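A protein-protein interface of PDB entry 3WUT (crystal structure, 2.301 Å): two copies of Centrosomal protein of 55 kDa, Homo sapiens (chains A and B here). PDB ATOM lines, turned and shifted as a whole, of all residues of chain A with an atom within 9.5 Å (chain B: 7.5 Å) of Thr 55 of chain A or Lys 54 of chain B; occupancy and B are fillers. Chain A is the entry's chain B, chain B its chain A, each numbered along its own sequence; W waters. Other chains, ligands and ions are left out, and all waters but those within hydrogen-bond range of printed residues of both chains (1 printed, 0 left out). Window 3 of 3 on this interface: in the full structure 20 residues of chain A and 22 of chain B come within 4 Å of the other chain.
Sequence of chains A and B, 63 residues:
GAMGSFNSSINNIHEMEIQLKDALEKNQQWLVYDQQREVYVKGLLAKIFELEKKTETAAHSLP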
ATOM      1  N   ILE A  48      11.478  -7.170  21.298  1.00  0.00           N
ATOM      2  CA  ILE A  48      11.520  -7.578  19.897  1.00  0.00           C
ATOM      3  C   ILE A  48      12.863  -8.222  19.570  1.00  0.00           C
ATOM      4  O   ILE A  48      12.926  -9.268  18.920  1.00  0.00           O
ATOM      5  CB  ILE A  48      11.296  -6.373  18.962  1.00  0.00           C
ATOM      6  CG1 ILE A  48       9.855  -5.871  19.082  1.00  0.00           C
ATOM      7  CG2 ILE A  48      11.642  -6.734  17.518  1.00  0.00           C
ATOM      8  CD1 ILE A  48       9.557  -4.607  18.308  1.00  0.00           C
ATOM      9  N   PHE A  49      13.934  -7.583  20.028  1.00  0.00           N
ATOM     10  CA  PHE A  49      15.281  -8.110  19.857  1.00  0.00           C
ATOM     11  C   PHE A  49      15.392  -9.541  20.395  1.00  0.00           C
ATOM     12  O   PHE A  49      15.904 -10.433  19.713  1.00  0.00           O
ATOM     13  CB  PHE A  49      16.288  -7.200  20.564  1.00  0.00           C
ATOM     14  CG  PHE A  49      17.704  -7.695  20.483  1.00  0.00           C
ATOM     15  CD1 PHE A  49      18.460  -7.489  19.342  1.00  0.00           C
ATOM     16  CD2 PHE A  49      18.277  -8.375  21.541  1.00  0.00           C
ATOM     17  CE1 PHE A  49      19.769  -7.958  19.257  1.00  0.00           C
ATOM     18  CE2 PHE A  49      19.581  -8.843  21.459  1.00  0.00           C
ATOM     19  CZ  PHE A  49      20.326  -8.632  20.315  1.00  0.00           C
ATOM     20  N   GLU A  50      14.901  -9.750  21.614  1.00  0.00           N
ATOM     21  CA  GLU A  50      14.940 -11.058  22.244  1.00  0.00           C
ATOM     22  C   GLU A  50      14.111 -12.064  21.460  1.00  0.00           C
ATOM     23  O   GLU A  50      14.553 -13.186  21.247  1.00  0.00           O
ATOM     24  CB  GLU A  50      14.464 -10.980  23.697  1.00  0.00           C
ATOM     25  CG  GLU A  50      15.338 -10.105  24.578  1.00  0.00           C
ATOM     26  CD  GLU A  50      16.783 -10.569  24.608  1.00  0.00           C
ATOM     27  OE1 GLU A  50      17.007 -11.794  24.670  1.00  0.00           O
ATOM     28  OE2 GLU A  50      17.698  -9.718  24.571  1.00  0.00           O
ATOM     29  N   LEU A  51      12.925 -11.653  21.015  1.00  0.00           N
ATOM     30  CA  LEU A  51      12.069 -12.515  20.208  1.00  0.00           C
ATOM     31  C   LEU A  51      12.668 -12.893  18.856  1.00  0.00           C
ATOM     32  O   LEU A  51      12.497 -14.018  18.397  1.00  0.00           O
ATOM     33  CB  LEU A  51      10.709 -11.860  19.989  1.00  0.00           C
ATOM     34  CG  LEU A  51       9.840 -11.827  21.243  1.00  0.00           C
ATOM     35  CD1 LEU A  51       8.585 -11.008  21.020  1.00  0.00           C
ATOM     36  CD2 LEU A  51       9.503 -13.253  21.706  1.00  0.00           C
ATOM     37  N   GLU A  52      13.352 -11.953  18.212  1.00  0.00           N
ATOM     38  CA  GLU A  52      13.950 -12.210  16.905  1.00  0.00           C
ATOM     39  C   GLU A  52      15.177 -13.085  17.061  1.00  0.00           C
ATOM     40  O   GLU A  52      15.554 -13.815  16.150  1.00  0.00           O
ATOM     41  CB  GLU A  52      14.338 -10.901  16.218  1.00  0.00           C
ATOM     42  CG  GLU A  52      13.137 -10.074  15.797  1.00  0.00           C
ATOM     43  CD  GLU A  52      13.531  -8.837  15.029  1.00  0.00           C
ATOM     44  OE1 GLU A  52      14.664  -8.351  15.216  1.00  0.00           O
ATOM     45  OE2 GLU A  52      12.710  -8.359  14.227  1.00  0.00           O
ATOM     46  N   LYS A  53      15.801 -12.989  18.228  1.00  0.00           N
ATOM     47  CA  LYS A  53      16.958 -13.798  18.564  1.00  0.00           C
ATOM     48  C   LYS A  53      16.527 -15.246  18.743  1.00  0.00           C
ATOM     49  O   LYS A  53      17.280 -16.163  18.436  1.00  0.00           O
ATOM     50  CB  LYS A  53      17.588 -13.276  19.853  1.00  0.00           C
ATOM     51  CG  LYS A  53      18.776 -14.073  20.343  1.00  0.00           C
ATOM     52  CD  LYS A  53      19.220 -13.606  21.717  1.00  0.00           C
ATOM     53  CE  LYS A  53      19.983 -12.296  21.632  1.00  0.00           C
ATOM     54  NZ  LYS A  53      21.288 -12.457  20.926  1.00  0.00           N
ATOM     55  N   LYS A  54      15.302 -15.434  19.230  1.00  0.00           N
ATOM     56  CA  LYS A  54      14.786 -16.759  19.549  1.00  0.00           C
ATOM     57  C   LYS A  54      14.636 -17.672  18.333  1.00  0.00           C
ATOM     58  O   LYS A  54      15.006 -18.845  18.393  1.00  0.00           O
ATOM     59  CB  LYS A  54      13.459 -16.656  20.305  1.00  0.00           C
ATOM     60  CG  LYS A  54      12.860 -18.008  20.660  1.00  0.00           C
ATOM     61  CD  LYS A  54      11.914 -17.918  21.846  1.00  0.00           C
ATOM     62  CE  LYS A  54      11.448 -19.305  22.276  1.00  0.00           C
ATOM     63  NZ  LYS A  54      10.658 -19.268  23.536  1.00  0.00           N
ATOM     64  N   THR A  55      14.092 -17.143  17.238  1.00  0.00           N
ATOM     65  CA  THR A  55      13.875 -17.939  16.027  1.00  0.00           C
ATOM     66  C   THR A  55      13.994 -17.131  14.726  1.00  0.00           C
ATOM     67  O   THR A  55      13.002 -16.527  14.317  1.00  0.00           O
ATOM     68  CB  THR A  55      12.474 -18.622  16.020  1.00  0.00           C
ATOM     69  OG1 THR A  55      11.476 -17.679  16.432  1.00  0.00           O
ATOM     70  CG2 THR A  55      12.434 -19.854  16.939  1.00  0.00           C
ATOM     71  N   GLU A  56      15.154 -17.096  14.052  1.00  0.00           N
ATOM     72  CA  GLU A  56      16.464 -17.634  14.469  1.00  0.00           C
ATOM     73  C   GLU A  56      16.549 -19.073  15.003  1.00  0.00           C
ATOM     74  O   GLU A  56      16.016 -20.004  14.398  1.00  0.00           O
ATOM     75  CB  GLU A  56      17.162 -16.667  15.434  1.00  0.00           C
ATOM     76  CG  GLU A  56      17.893 -15.510  14.762  1.00  0.00           C
ATOM     77  CD  GLU A  56      19.369 -15.498  15.095  1.00  0.00           C
ATOM     78  OE1 GLU A  56      19.826 -16.429  15.794  1.00  0.00           O
ATOM     79  OE2 GLU A  56      20.070 -14.562  14.655  1.00  0.00           O
ATOM     80  N   THR A  57      17.225 -19.226  16.142  1.00  0.00           N
ATOM     81  CA  THR A  57      17.349 -20.509  16.833  1.00  0.00           C
ATOM     82  C   THR A  57      17.616 -20.306  18.326  1.00  0.00           C
ATOM     83  O   THR A  57      16.843 -20.752  19.178  1.00  0.00           O
ATOM     84  CB  THR A  57      18.481 -21.375  16.238  1.00  0.00           C
ATOM     85  OG1 THR A  57      19.492 -20.526  15.676  1.00  0.00           O
ATOM     86  CG2 THR A  57      17.942 -22.312  15.160  1.00  0.00           C
ATOM     87  N   ILE B  48       5.380  -7.405  17.933  1.00  0.00           N
ATOM     88  CA  ILE B  48       5.586  -8.337  19.032  1.00  0.00           C
ATOM     89  C   ILE B  48       4.561  -9.463  19.012  1.00  0.00           C
ATOM     90  O   ILE B  48       4.910 -10.622  19.202  1.00  0.00           O
ATOM     91  CB  ILE B  48       5.526  -7.617  20.376  1.00  0.00           C
ATOM     92  CG1 ILE B  48       6.737  -6.702  20.504  1.00  0.00           C
ATOM     93  CG2 ILE B  48       5.476  -8.622  21.533  1.00  0.00           C
ATOM     94  CD1 ILE B  48       6.681  -5.754  21.672  1.00  0.00           C
ATOM     95  N   PHE B  49       3.305  -9.113  18.769  1.00  0.00           N
ATOM     96  CA  PHE B  49       2.227 -10.092  18.710  1.00  0.00           C
ATOM     97  C   PHE B  49       2.460 -11.157  17.634  1.00  0.00           C
ATOM     98  O   PHE B  49       2.116 -12.327  17.829  1.00  0.00           O
ATOM     99  CB  PHE B  49       0.889  -9.383  18.480  1.00  0.00           C
ATOM    100  CG  PHE B  49      -0.284 -10.317  18.431  1.00  0.00           C
ATOM    101  CD1 PHE B  49      -0.956 -10.665  19.596  1.00  0.00           C
ATOM    102  CD2 PHE B  49      -0.708 -10.867  17.226  1.00  0.00           C
ATOM    103  CE1 PHE B  49      -2.031 -11.537  19.557  1.00  0.00           C
ATOM    104  CE2 PHE B  49      -1.787 -11.743  17.188  1.00  0.00           C
ATOM    105  CZ  PHE B  49      -2.448 -12.077  18.355  1.00  0.00           C
ATOM    106  N   GLU B  50       3.038 -10.749  16.505  1.00  0.00           N
ATOM    107  CA  GLU B  50       3.340 -11.670  15.411  1.00  0.00           C
ATOM    108  C   GLU B  50       4.608 -12.470  15.663  1.00  0.00           C
ATOM    109  O   GLU B  50       4.737 -13.596  15.190  1.00  0.00           O
ATOM    110  CB  GLU B  50       3.483 -10.920  14.088  1.00  0.00           C
ATOM    111  CG  GLU B  50       2.240 -10.163  13.659  1.00  0.00           C
ATOM    112  CD  GLU B  50       1.019 -11.055  13.495  1.00  0.00           C
ATOM    113  OE1 GLU B  50      -0.093 -10.563  13.756  1.00  0.00           O
ATOM    114  OE2 GLU B  50       1.163 -12.232  13.095  1.00  0.00           O
ATOM    115  N   LEU B  51       5.551 -11.887  16.393  1.00  0.00           N
ATOM    116  CA  LEU B  51       6.774 -12.606  16.736  1.00  0.00           C
ATOM    117  C   LEU B  51       6.502 -13.655  17.806  1.00  0.00           C
ATOM    118  O   LEU B  51       7.057 -14.745  17.763  1.00  0.00           O
ATOM    119  CB  LEU B  51       7.864 -11.647  17.203  1.00  0.00           C
ATOM    120  CG  LEU B  51       8.652 -10.940  16.099  1.00  0.00           C
ATOM    121  CD1 LEU B  51       9.448  -9.783  16.674  1.00  0.00           C
ATOM    122  CD2 LEU B  51       9.562 -11.927  15.357  1.00  0.00           C
ATOM    123  N   GLU B  52       5.645 -13.317  18.761  1.00  0.00           N
ATOM    124  CA  GLU B  52       5.262 -14.252  19.806  1.00  0.00           C
ATOM    125  C   GLU B  52       4.489 -15.404  19.189  1.00  0.00           C
ATOM    126  O   GLU B  52       4.678 -16.559  19.560  1.00  0.00           O
ATOM    127  CB  GLU B  52       4.430 -13.552  20.875  1.00  0.00           C
ATOM    128  CG  GLU B  52       5.275 -12.670  21.770  1.00  0.00           C
ATOM    129  CD  GLU B  52       4.459 -11.916  22.780  1.00  0.00           C
ATOM    130  OE1 GLU B  52       3.245 -11.738  22.548  1.00  0.00           O
ATOM    131  OE2 GLU B  52       5.029 -11.501  23.805  1.00  0.00           O
ATOM    132  N   LYS B  53       3.638 -15.082  18.228  1.00  0.00           N
ATOM    133  CA  LYS B  53       2.894 -16.085  17.497  1.00  0.00           C
ATOM    134  C   LYS B  53       3.840 -16.978  16.713  1.00  0.00           C
ATOM    135  O   LYS B  53       3.595 -18.174  16.572  1.00  0.00           O
ATOM    136  CB  LYS B  53       1.921 -15.412  16.538  1.00  0.00           C
ATOM    137  CG  LYS B  53       1.133 -16.375  15.682  1.00  0.00           C
ATOM    138  CD  LYS B  53       0.251 -15.623  14.712  1.00  0.00           C
ATOM    139  CE  LYS B  53      -0.757 -14.764  15.451  1.00  0.00           C
ATOM    140  NZ  LYS B  53      -1.882 -15.568  16.006  1.00  0.00           N
ATOM    141  N   LYS B  54       4.924 -16.398  16.210  1.00  0.00           N
ATOM    142  CA  LYS B  54       5.846 -17.155  15.379  1.00  0.00           C
ATOM    143  C   LYS B  54       6.744 -18.054  16.223  1.00  0.00           C
ATOM    144  O   LYS B  54       7.091 -19.155  15.802  1.00  0.00           O
ATOM    145  CB  LYS B  54       6.684 -16.229  14.499  1.00  0.00           C
ATOM    146  CG  LYS B  54       7.188 -16.898  13.234  1.00  0.00           C
ATOM    147  CD  LYS B  54       8.309 -16.110  12.580  1.00  0.00           C
ATOM    148  CE  LYS B  54       9.611 -16.265  13.349  1.00  0.00           C
ATOM    149  NZ  LYS B  54      10.775 -15.659  12.628  1.00  0.00           N
ATOM    150  N   THR B  55       7.103 -17.590  17.417  1.00  0.00           N
ATOM    151  CA  THR B  55       7.958 -18.363  18.309  1.00  0.00           C
ATOM    152  C   THR B  55       7.176 -19.445  19.060  1.00  0.00           C
ATOM    153  O   THR B  55       7.769 -20.286  19.736  1.00  0.00           O
ATOM    154  CB  THR B  55       8.711 -17.462  19.326  1.00  0.00           C
ATOM    155  OG1 THR B  55       7.768 -16.757  20.146  1.00  0.00           O
ATOM    156  CG2 THR B  55       9.620 -16.461  18.604  1.00  0.00           C
ATOM    157  N   GLU B  56       5.852 -19.427  18.938  1.00  0.00           N
ATOM    158  CA  GLU B  56       5.024 -20.468  19.540  1.00  0.00           C
ATOM    159  C   GLU B  56       4.933 -21.697  18.637  1.00  0.00           C
ATOM    160  O   GLU B  56       4.881 -22.827  19.123  1.00  0.00           O
ATOM    161  CB  GLU B  56       3.627 -19.943  19.841  1.00  0.00           C
ATOM    162  CG  GLU B  56       3.565 -19.024  21.040  1.00  0.00           C
ATOM    163  CD  GLU B  56       2.258 -18.260  21.099  1.00  0.00           C
ATOM    164  OE1 GLU B  56       1.249 -18.774  20.562  1.00  0.00           O
ATOM    165  OE2 GLU B  56       2.245 -17.143  21.671  1.00  0.00           O
ATOM    166  N   THR B  57       4.918 -21.472  17.326  1.00  0.00           N
ATOM    167  CA  THR B  57       4.820 -22.570  16.369  1.00  0.00           C
ATOM    168  C   THR B  57       6.179 -23.229  16.144  1.00  0.00           C
ATOM    169  O   THR B  57       6.849 -23.624  17.098  1.00  0.00           O
ATOM    170  CB  THR B  57       4.242 -22.106  15.010  1.00  0.00           C
ATOM    171  OG1 THR B  57       3.143 -21.209  15.226  1.00  0.00           O
ATOM    172  CG2 THR B  57       3.769 -23.310  14.193  1.00  0.00           C
HETATM  173  O   HOH W   1      12.117 -13.518  13.306  1.00  0.00           O
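Of the 10 printed residues of chain A, 4 touch a printed residue of chain B.
Of the 10 printed residues of chain B, 5 touch a printed residue of chain A.
Hydrophobic or aromatic side chains of chain B within 4 Å of the printed part of chain A: Ile 48 and Leu 51.
Among the printed residues, 9 pairs touch across the chains.
Among the printed residues, no Asp or Glu carboxylate lies within 4 Å of a Lys or Arg side-chain nitrogen of the other chain.
Water W1 bridges the side-chain amino group (NZ) of Lys 54 of chain B (2.6 Å) and the backbone carbonyl oxygen (O) of Thr 55 of chain A (3.3 Å).
The backbone carbonyl oxygen (O) of Leu 51 of chain B lies close to the side-chain hydroxyl (OG1) of Thr 55 of chain B (3.2 Å).
The backbone carbonyl oxygen (O) of Glu 52 of chain B lies within hydrogen-bond range of the side-chain hydroxyl (OG1) of Thr 55 of chain B (3.2 Å).
Thr 55 of chain A touches just these residues of chain B: Lys 54 (2.9 Å) and Thr 55 (3.1 Å).
Of the printed residues of chain A, Leu 51 of chain B touches Ile 48, Leu 51 and Glu 52.
Of the printed residues of chain B, Glu 52 of chain A touches Leu 51 (3.8 Å).
Of the printed residues of chain A, Ile 48 of chain B touches Ile 48 (3.5 Å) and Leu 51 (3.95 Å).
Glu 50 of chain A touches none of the printed residues of chain B.
The nearest residue of chain B that does not touch Thr 55 of chain A is Leu 51 of chain B (5.5 Å).
Ile 48 of chain A touches Leu 51 of chain B, and with the chains exchanged Leu 51 of chain A touches Ile 48 of chain B.
Leu 51 of chain A touches Glu 52 of chain B, and with the chains exchanged Glu 52 of chain A touches Leu 51 of chain B.
Leu 51 of chain A touches Thr 55 of chain B, but with the chains exchanged Thr 55 of chain A does not touch Leu 51 of chain B (5.5 Å).
Thr 55 of chain A touches Lys 54 of chain B, but with the chains exchanged Lys 54 of chain A does not touch Thr 55 of chain B (4.1 Å).
Ile 48 of chain A touches Ile 48 of chain B (CG1 to CG1, 3.5 Å).
Ile 48 of chain A touches Leu 51 of chain B.
Ile 48 of chain B touches Leu 51 of chain A (CG2 to CD1, 3.95 Å).
Leu 51 of chain B touches Leu 51 of chain A.
Glu 52 of chain B touches Leu 51 of chain A.
O of Leu 51 of chain A touches CG2 of Thr 55 of chain B, at 3.8 Å.
Leu 51 of chain B touches Glu 52 of chain A.
Thr 55 of chain B touches Thr 55 of chain A.
NZ of Lys 54 of chain B is in hydrogen-bond range of O of Thr 55 of chain A, at 2.9 Å.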
